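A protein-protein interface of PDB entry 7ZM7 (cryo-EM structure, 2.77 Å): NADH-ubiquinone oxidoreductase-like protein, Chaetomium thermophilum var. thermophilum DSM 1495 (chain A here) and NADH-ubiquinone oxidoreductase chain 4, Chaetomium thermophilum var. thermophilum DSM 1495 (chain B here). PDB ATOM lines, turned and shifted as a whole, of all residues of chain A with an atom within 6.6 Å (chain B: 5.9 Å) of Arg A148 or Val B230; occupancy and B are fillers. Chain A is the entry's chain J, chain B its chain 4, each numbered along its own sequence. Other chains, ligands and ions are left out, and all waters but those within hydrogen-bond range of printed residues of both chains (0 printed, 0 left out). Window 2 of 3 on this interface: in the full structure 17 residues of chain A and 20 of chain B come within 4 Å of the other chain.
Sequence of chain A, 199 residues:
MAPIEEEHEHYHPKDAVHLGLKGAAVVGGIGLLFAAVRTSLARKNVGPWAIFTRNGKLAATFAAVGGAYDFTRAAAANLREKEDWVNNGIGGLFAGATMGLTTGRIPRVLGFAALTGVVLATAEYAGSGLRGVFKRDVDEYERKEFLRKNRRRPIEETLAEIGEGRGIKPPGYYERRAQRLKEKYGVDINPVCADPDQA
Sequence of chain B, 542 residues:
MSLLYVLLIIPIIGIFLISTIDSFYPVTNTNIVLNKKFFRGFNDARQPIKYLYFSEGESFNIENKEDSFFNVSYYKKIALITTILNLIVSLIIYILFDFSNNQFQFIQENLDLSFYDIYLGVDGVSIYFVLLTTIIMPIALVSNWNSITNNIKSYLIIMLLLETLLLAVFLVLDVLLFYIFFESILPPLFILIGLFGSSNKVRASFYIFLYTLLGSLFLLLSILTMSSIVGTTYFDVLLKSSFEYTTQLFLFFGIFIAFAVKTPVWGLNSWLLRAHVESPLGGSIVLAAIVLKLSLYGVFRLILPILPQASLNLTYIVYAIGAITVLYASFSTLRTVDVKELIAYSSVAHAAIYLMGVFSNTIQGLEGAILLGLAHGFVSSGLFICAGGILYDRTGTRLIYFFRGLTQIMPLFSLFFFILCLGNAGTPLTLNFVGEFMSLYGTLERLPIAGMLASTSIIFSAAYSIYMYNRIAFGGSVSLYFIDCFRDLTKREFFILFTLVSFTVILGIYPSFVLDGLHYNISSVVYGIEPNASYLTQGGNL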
ATOM      1  N   ARG A 143      13.030  -9.956  19.162  1.00  0.00           N
ATOM      2  CA  ARG A 143      13.146 -10.674  20.461  1.00  0.00           C
ATOM      3  C   ARG A 143      13.270  -9.676  21.615  1.00  0.00           C
ATOM      4  O   ARG A 143      12.556  -9.842  22.615  1.00  0.00           O
ATOM      5  CB  ARG A 143      14.327 -11.645  20.415  1.00  0.00           C
ATOM      6  CG  ARG A 143      14.678 -12.271  21.755  1.00  0.00           C
ATOM      7  CD  ARG A 143      15.827 -13.249  21.630  1.00  0.00           C
ATOM      8  NE  ARG A 143      16.332 -13.672  22.927  1.00  0.00           N
ATOM      9  CZ  ARG A 143      15.905 -14.739  23.593  1.00  0.00           C
ATOM     10  NH1 ARG A 143      14.955 -15.502  23.083  1.00  0.00           N
ATOM     11  NH2 ARG A 143      16.432 -15.038  24.766  1.00  0.00           N
ATOM     12  N   LYS A 144      14.120  -8.661  21.451  1.00  0.00           N
ATOM     13  CA  LYS A 144      14.336  -7.644  22.505  1.00  0.00           C
ATOM     14  C   LYS A 144      13.070  -6.815  22.680  1.00  0.00           C
ATOM     15  O   LYS A 144      12.675  -6.595  23.829  1.00  0.00           O
ATOM     16  CB  LYS A 144      15.573  -6.815  22.160  1.00  0.00           C
ATOM     17  CG  LYS A 144      16.906  -7.385  22.623  1.00  0.00           C
ATOM     18  CD  LYS A 144      17.089  -7.310  24.122  1.00  0.00           C
ATOM     19  CE  LYS A 144      18.523  -7.525  24.556  1.00  0.00           C
ATOM     20  NZ  LYS A 144      19.047  -8.837  24.109  1.00  0.00           N
ATOM     21  N   GLU A 145      12.448  -6.406  21.578  1.00  0.00           N
ATOM     22  CA  GLU A 145      11.246  -5.534  21.649  1.00  0.00           C
ATOM     23  C   GLU A 145      10.063  -6.276  22.275  1.00  0.00           C
ATOM     24  O   GLU A 145       9.279  -5.631  22.983  1.00  0.00           O
ATOM     25  CB  GLU A 145      10.947  -4.876  20.303  1.00  0.00           C
ATOM     26  CG  GLU A 145      11.865  -3.716  19.971  1.00  0.00           C
ATOM     27  CD  GLU A 145      11.567  -2.433  20.724  1.00  0.00           C
ATOM     28  OE1 GLU A 145      10.684  -1.684  20.275  1.00  0.00           O
ATOM     29  OE2 GLU A 145      12.214  -2.186  21.754  1.00  0.00           O
ATOM     30  N   PHE A 146       9.920  -7.569  21.995  1.00  0.00           N
ATOM     31  CA  PHE A 146       8.837  -8.355  22.631  1.00  0.00           C
ATOM     32  C   PHE A 146       9.040  -8.392  24.139  1.00  0.00           C
ATOM     33  O   PHE A 146       8.065  -8.220  24.868  1.00  0.00           O
ATOM     34  CB  PHE A 146       8.786  -9.794  22.118  1.00  0.00           C
ATOM     35  CG  PHE A 146       7.802 -10.658  22.862  1.00  0.00           C
ATOM     36  CD1 PHE A 146       6.438 -10.470  22.708  1.00  0.00           C
ATOM     37  CD2 PHE A 146       8.234 -11.638  23.740  1.00  0.00           C
ATOM     38  CE1 PHE A 146       5.529 -11.248  23.406  1.00  0.00           C
ATOM     39  CE2 PHE A 146       7.326 -12.412  24.441  1.00  0.00           C
ATOM     40  CZ  PHE A 146       5.975 -12.219  24.270  1.00  0.00           C
ATOM     41  N   LEU A 147      10.274  -8.585  24.588  1.00  0.00           N
ATOM     42  CA  LEU A 147      10.490  -8.744  26.043  1.00  0.00           C
ATOM     43  C   LEU A 147      10.435  -7.382  26.743  1.00  0.00           C
ATOM     44  O   LEU A 147      10.348  -7.377  27.965  1.00  0.00           O
ATOM     45  CB  LEU A 147      11.809  -9.490  26.246  1.00  0.00           C
ATOM     46  CG  LEU A 147      11.795 -10.969  25.877  1.00  0.00           C
ATOM     47  CD1 LEU A 147      13.167 -11.581  26.088  1.00  0.00           C
ATOM     48  CD2 LEU A 147      10.753 -11.713  26.693  1.00  0.00           C
ATOM     49  N   ARG A 148      10.460  -6.277  26.000  1.00  0.00           N
ATOM     50  CA  ARG A 148      10.327  -4.920  26.596  1.00  0.00           C
ATOM     51  C   ARG A 148       8.844  -4.529  26.686  1.00  0.00           C
ATOM     52  O   ARG A 148       8.459  -3.889  27.676  1.00  0.00           O
ATOM     53  CB  ARG A 148      11.084  -3.900  25.734  1.00  0.00           C
ATOM     54  CG  ARG A 148      10.906  -2.456  26.187  1.00  0.00           C
ATOM     55  CD  ARG A 148      11.614  -1.408  25.352  1.00  0.00           C
ATOM     56  NE  ARG A 148      11.006  -1.123  24.061  1.00  0.00           N
ATOM     57  CZ  ARG A 148      10.104  -0.175  23.845  1.00  0.00           C
ATOM     58  NH1 ARG A 148       9.617   0.009  22.632  1.00  0.00           N
ATOM     59  NH2 ARG A 148       9.690   0.587  24.839  1.00  0.00           N
ATOM     60  N   LYS A 149       8.044  -4.895  25.689  1.00  0.00           N
ATOM     61  CA  LYS A 149       6.632  -4.557  25.670  1.00  0.00           C
ATOM     62  C   LYS A 149       5.732  -5.698  26.109  1.00  0.00           C
ATOM     63  O   LYS A 149       4.517  -5.614  25.926  1.00  0.00           O
ATOM     64  CB  LYS A 149       6.237  -4.058  24.288  1.00  0.00           C
ATOM     65  CG  LYS A 149       6.907  -2.765  23.924  1.00  0.00           C
ATOM     66  CD  LYS A 149       6.393  -2.238  22.601  1.00  0.00           C
ATOM     67  CE  LYS A 149       6.867  -3.063  21.426  1.00  0.00           C
ATOM     68  NZ  LYS A 149       8.315  -2.935  21.225  1.00  0.00           N
ATOM     69  N   ASN A 150       6.288  -6.744  26.705  1.00  0.00           N
ATOM     70  CA  ASN A 150       5.494  -7.853  27.233  1.00  0.00           C
ATOM     71  C   ASN A 150       5.061  -7.565  28.669  1.00  0.00           C
ATOM     72  O   ASN A 150       5.323  -8.313  29.603  1.00  0.00           O
ATOM     73  CB  ASN A 150       6.285  -9.146  27.141  1.00  0.00           C
ATOM     74  CG  ASN A 150       5.477 -10.337  27.520  1.00  0.00           C
ATOM     75  OD1 ASN A 150       4.258 -10.328  27.406  1.00  0.00           O
ATOM     76  ND2 ASN A 150       6.149 -11.383  27.991  1.00  0.00           N
ATOM     77  N   ARG A 151       4.366  -6.447  28.823  1.00  0.00           N
ATOM     78  CA  ARG A 151       4.143  -5.880  30.144  1.00  0.00           C
ATOM     79  C   ARG A 151       3.100  -6.647  30.945  1.00  0.00           C
ATOM     80  O   ARG A 151       3.186  -6.687  32.175  1.00  0.00           O
ATOM     81  CB  ARG A 151       3.759  -4.413  29.993  1.00  0.00           C
ATOM     82  CG  ARG A 151       4.699  -3.649  29.090  1.00  0.00           C
ATOM     83  CD  ARG A 151       4.933  -2.246  29.606  1.00  0.00           C
ATOM     84  NE  ARG A 151       6.129  -1.608  29.059  1.00  0.00           N
ATOM     85  CZ  ARG A 151       6.148  -0.799  28.001  1.00  0.00           C
ATOM     86  NH1 ARG A 151       7.287  -0.260  27.605  1.00  0.00           N
ATOM     87  NH2 ARG A 151       5.044  -0.529  27.333  1.00  0.00           N
ATOM     88  N   THR B 225      21.992  -6.543  32.760  1.00  0.00           N
ATOM     89  CA  THR B 225      20.993  -7.377  32.101  1.00  0.00           C
ATOM     90  C   THR B 225      19.643  -6.675  32.002  1.00  0.00           C
ATOM     91  O   THR B 225      18.990  -6.706  30.957  1.00  0.00           O
ATOM     92  CB  THR B 225      20.847  -8.693  32.854  1.00  0.00           C
ATOM     93  OG1 THR B 225      22.119  -9.337  32.913  1.00  0.00           O
ATOM     94  CG2 THR B 225      19.875  -9.597  32.146  1.00  0.00           C
ATOM     95  N   MET B 226      19.201  -6.047  33.083  1.00  0.00           N
ATOM     96  CA  MET B 226      17.918  -5.359  33.052  1.00  0.00           C
ATOM     97  C   MET B 226      17.912  -4.254  32.004  1.00  0.00           C
ATOM     98  O   MET B 226      16.933  -4.087  31.271  1.00  0.00           O
ATOM     99  CB  MET B 226      17.621  -4.770  34.426  1.00  0.00           C
ATOM    100  CG  MET B 226      17.389  -5.784  35.490  1.00  0.00           C
ATOM    101  SD  MET B 226      17.065  -5.041  37.078  1.00  0.00           S
ATOM    102  CE  MET B 226      16.944  -6.497  38.101  1.00  0.00           C
ATOM    103  N   SER B 227      18.996  -3.482  31.931  1.00  0.00           N
ATOM    104  CA  SER B 227      19.072  -2.392  30.971  1.00  0.00           C
ATOM    105  C   SER B 227      19.050  -2.905  29.545  1.00  0.00           C
ATOM    106  O   SER B 227      18.392  -2.320  28.683  1.00  0.00           O
ATOM    107  CB  SER B 227      20.328  -1.575  31.212  1.00  0.00           C
ATOM    108  OG  SER B 227      20.507  -0.610  30.193  1.00  0.00           O
ATOM    109  N   SER B 228      19.776  -3.987  29.271  1.00  0.00           N
ATOM    110  CA  SER B 228      19.811  -4.523  27.916  1.00  0.00           C
ATOM    111  C   SER B 228      18.438  -5.001  27.471  1.00  0.00           C
ATOM    112  O   SER B 228      18.019  -4.738  26.343  1.00  0.00           O
ATOM    113  CB  SER B 228      20.827  -5.656  27.830  1.00  0.00           C
ATOM    114  OG  SER B 228      20.322  -6.812  28.456  1.00  0.00           O
ATOM    115  N   ILE B 229      17.716  -5.689  28.348  1.00  0.00           N
ATOM    116  CA  ILE B 229      16.372  -6.153  28.029  1.00  0.00           C
ATOM    117  C   ILE B 229      15.412  -4.987  27.839  1.00  0.00           C
ATOM    118  O   ILE B 229      14.629  -4.967  26.890  1.00  0.00           O
ATOM    119  CB  ILE B 229      15.880  -7.115  29.125  1.00  0.00           C
ATOM    120  CG1 ILE B 229      16.753  -8.369  29.152  1.00  0.00           C
ATOM    121  CG2 ILE B 229      14.411  -7.457  28.923  1.00  0.00           C
ATOM    122  CD1 ILE B 229      16.596  -9.227  30.379  1.00  0.00           C
ATOM    123  N   VAL B 230      15.457  -3.999  28.725  1.00  0.00           N
ATOM    124  CA  VAL B 230      14.469  -2.930  28.712  1.00  0.00           C
ATOM    125  C   VAL B 230      14.922  -1.721  27.889  1.00  0.00           C
ATOM    126  O   VAL B 230      14.090  -1.007  27.330  1.00  0.00           O
ATOM    127  CB  VAL B 230      14.127  -2.531  30.160  1.00  0.00           C
ATOM    128  CG1 VAL B 230      13.209  -1.342  30.199  1.00  0.00           C
ATOM    129  CG2 VAL B 230      13.475  -3.660  30.874  1.00  0.00           C
ATOM    130  N   GLY B 231      16.217  -1.472  27.795  1.00  0.00           N
ATOM    131  CA  GLY B 231      16.740  -0.357  27.050  1.00  0.00           C
ATOM    132  C   GLY B 231      17.141   0.830  27.894  1.00  0.00           C
ATOM    133  O   GLY B 231      17.897   1.678  27.424  1.00  0.00           O
ATOM    134  N   THR B 232      16.660   0.906  29.123  1.00  0.00           N
ATOM    135  CA  THR B 232      17.028   1.976  30.029  1.00  0.00           C
ATOM    136  C   THR B 232      16.949   1.442  31.449  1.00  0.00           C
ATOM    137  O   THR B 232      16.495   0.324  31.691  1.00  0.00           O
ATOM    138  CB  THR B 232      16.144   3.226  29.808  1.00  0.00           C
ATOM    139  OG1 THR B 232      16.566   4.291  30.669  1.00  0.00           O
ATOM    140  CG2 THR B 232      14.682   2.942  30.030  1.00  0.00           C
ATOM    141  N   VAL B 237      10.396   3.483  33.439  1.00  0.00           N
ATOM    142  CA  VAL B 237      10.310   2.523  32.354  1.00  0.00           C
ATOM    143  C   VAL B 237      10.536   1.099  32.854  1.00  0.00           C
ATOM    144  O   VAL B 237       9.965   0.158  32.302  1.00  0.00           O
ATOM    145  CB  VAL B 237      11.304   2.908  31.245  1.00  0.00           C
ATOM    146  CG1 VAL B 237      11.295   1.891  30.116  1.00  0.00           C
ATOM    147  CG2 VAL B 237      11.027   4.295  30.733  1.00  0.00           C
ATOM    148  N   LEU B 238      11.350   0.922  33.900  1.00  0.00           N
ATOM    149  CA  LEU B 238      11.527  -0.389  34.530  1.00  0.00           C
ATOM    150  C   LEU B 238      10.284  -0.885  35.250  1.00  0.00           C
ATOM    151  O   LEU B 238       9.980  -2.078  35.208  1.00  0.00           O
ATOM    152  CB  LEU B 238      12.693  -0.366  35.512  1.00  0.00           C
ATOM    153  CG  LEU B 238      14.116  -0.189  35.033  1.00  0.00           C
ATOM    154  CD1 LEU B 238      15.011  -0.057  36.212  1.00  0.00           C
ATOM    155  CD2 LEU B 238      14.474  -1.474  34.324  1.00  0.00           C
ATOM    156  N   SER B 241       7.870  -2.449  33.050  1.00  0.00           N
ATOM    157  CA  SER B 241       8.289  -3.738  32.453  1.00  0.00           C
ATOM    158  C   SER B 241       8.237  -4.923  33.416  1.00  0.00           C
ATOM    159  O   SER B 241       8.694  -4.776  34.556  1.00  0.00           O
ATOM    160  CB  SER B 241       9.653  -3.558  31.870  1.00  0.00           C
ATOM    161  OG  SER B 241       9.624  -2.593  30.829  1.00  0.00           O
ATOM    162  N   SER B 242       7.707  -6.053  32.955  1.00  0.00           N
ATOM    163  CA  SER B 242       7.724  -7.276  33.787  1.00  0.00           C
ATOM    164  C   SER B 242       8.634  -8.344  33.169  1.00  0.00           C
ATOM    165  O   SER B 242       8.294  -8.876  32.105  1.00  0.00           O
ATOM    166  CB  SER B 242       6.346  -7.783  34.019  1.00  0.00           C
ATOM    167  OG  SER B 242       6.373  -8.979  34.785  1.00  0.00           O
ATOM    168  N   PHE B 243       9.698  -8.706  33.874  1.00  0.00           N
ATOM    169  CA  PHE B 243      10.662  -9.715  33.397  1.00  0.00           C
ATOM    170  C   PHE B 243      10.074 -11.113  33.490  1.00  0.00           C
ATOM    171  O   PHE B 243       9.191 -11.316  34.305  1.00  0.00           O
ATOM    172  CB  PHE B 243      11.957  -9.600  34.194  1.00  0.00           C
ATOM    173  CG  PHE B 243      12.682  -8.291  34.031  1.00  0.00           C
ATOM    174  CD1 PHE B 243      12.480  -7.254  34.926  1.00  0.00           C
ATOM    175  CD2 PHE B 243      13.570  -8.100  32.986  1.00  0.00           C
ATOM    176  CE1 PHE B 243      13.147  -6.051  34.774  1.00  0.00           C
ATOM    177  CE2 PHE B 243      14.238  -6.896  32.838  1.00  0.00           C
ATOM    178  CZ  PHE B 243      14.024  -5.875  33.731  1.00  0.00           C
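Of the 13 printed residues of chain B, 5 touch a printed residue of chain A.
Among the printed residues, 7 pairs touch across the chains.
OE2 of Glu A145 lies within salt-bridge range of NE of Arg A148.
O of Thr B225 is in hydrogen-bond range of OG of Ser B228, at 2.8 Å.
OG of Ser B241 sits at hydrogen-bond distance from O of Val B237, 3.1 Å away.
Among the printed residues, merely in contact across the chains: Lys A144 with Ser B228 (3.3 Å), Lys A144 with Ile B229 (3.98 Å), Arg A148 with Ile B229 (3.9 Å), Arg A148 with Val B230 (3.2 Å), Arg A148 with Ser B241 (3.6 Å), Asn A150 with Ser B242 (3.9 Å) and Arg A151 with Ser B242 (3.8 Å).
Of chain B, only Ile B229, Val B230 and Ser B241 come within 4 Å of Arg A148.
Of chain A, only Arg A148 (3.2 Å) comes within 4 Å of Val B230.
Of the printed residues of chain B, Asn A150 touches Ser B242.
Of the printed residues of chain A, Ser B242 touches Asn A150 (3.9 Å) and Arg A151 (3.8 Å).
The nearest residue of chain B that does not touch Arg A148 is Gly B231 (5.2 Å).
The nearest residue of chain A that does not touch Val B230 is Leu A147 (5.7 Å).
The nearest printed residue of chain A that does not touch Ser B228 is Arg A148 (7.0 Å).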
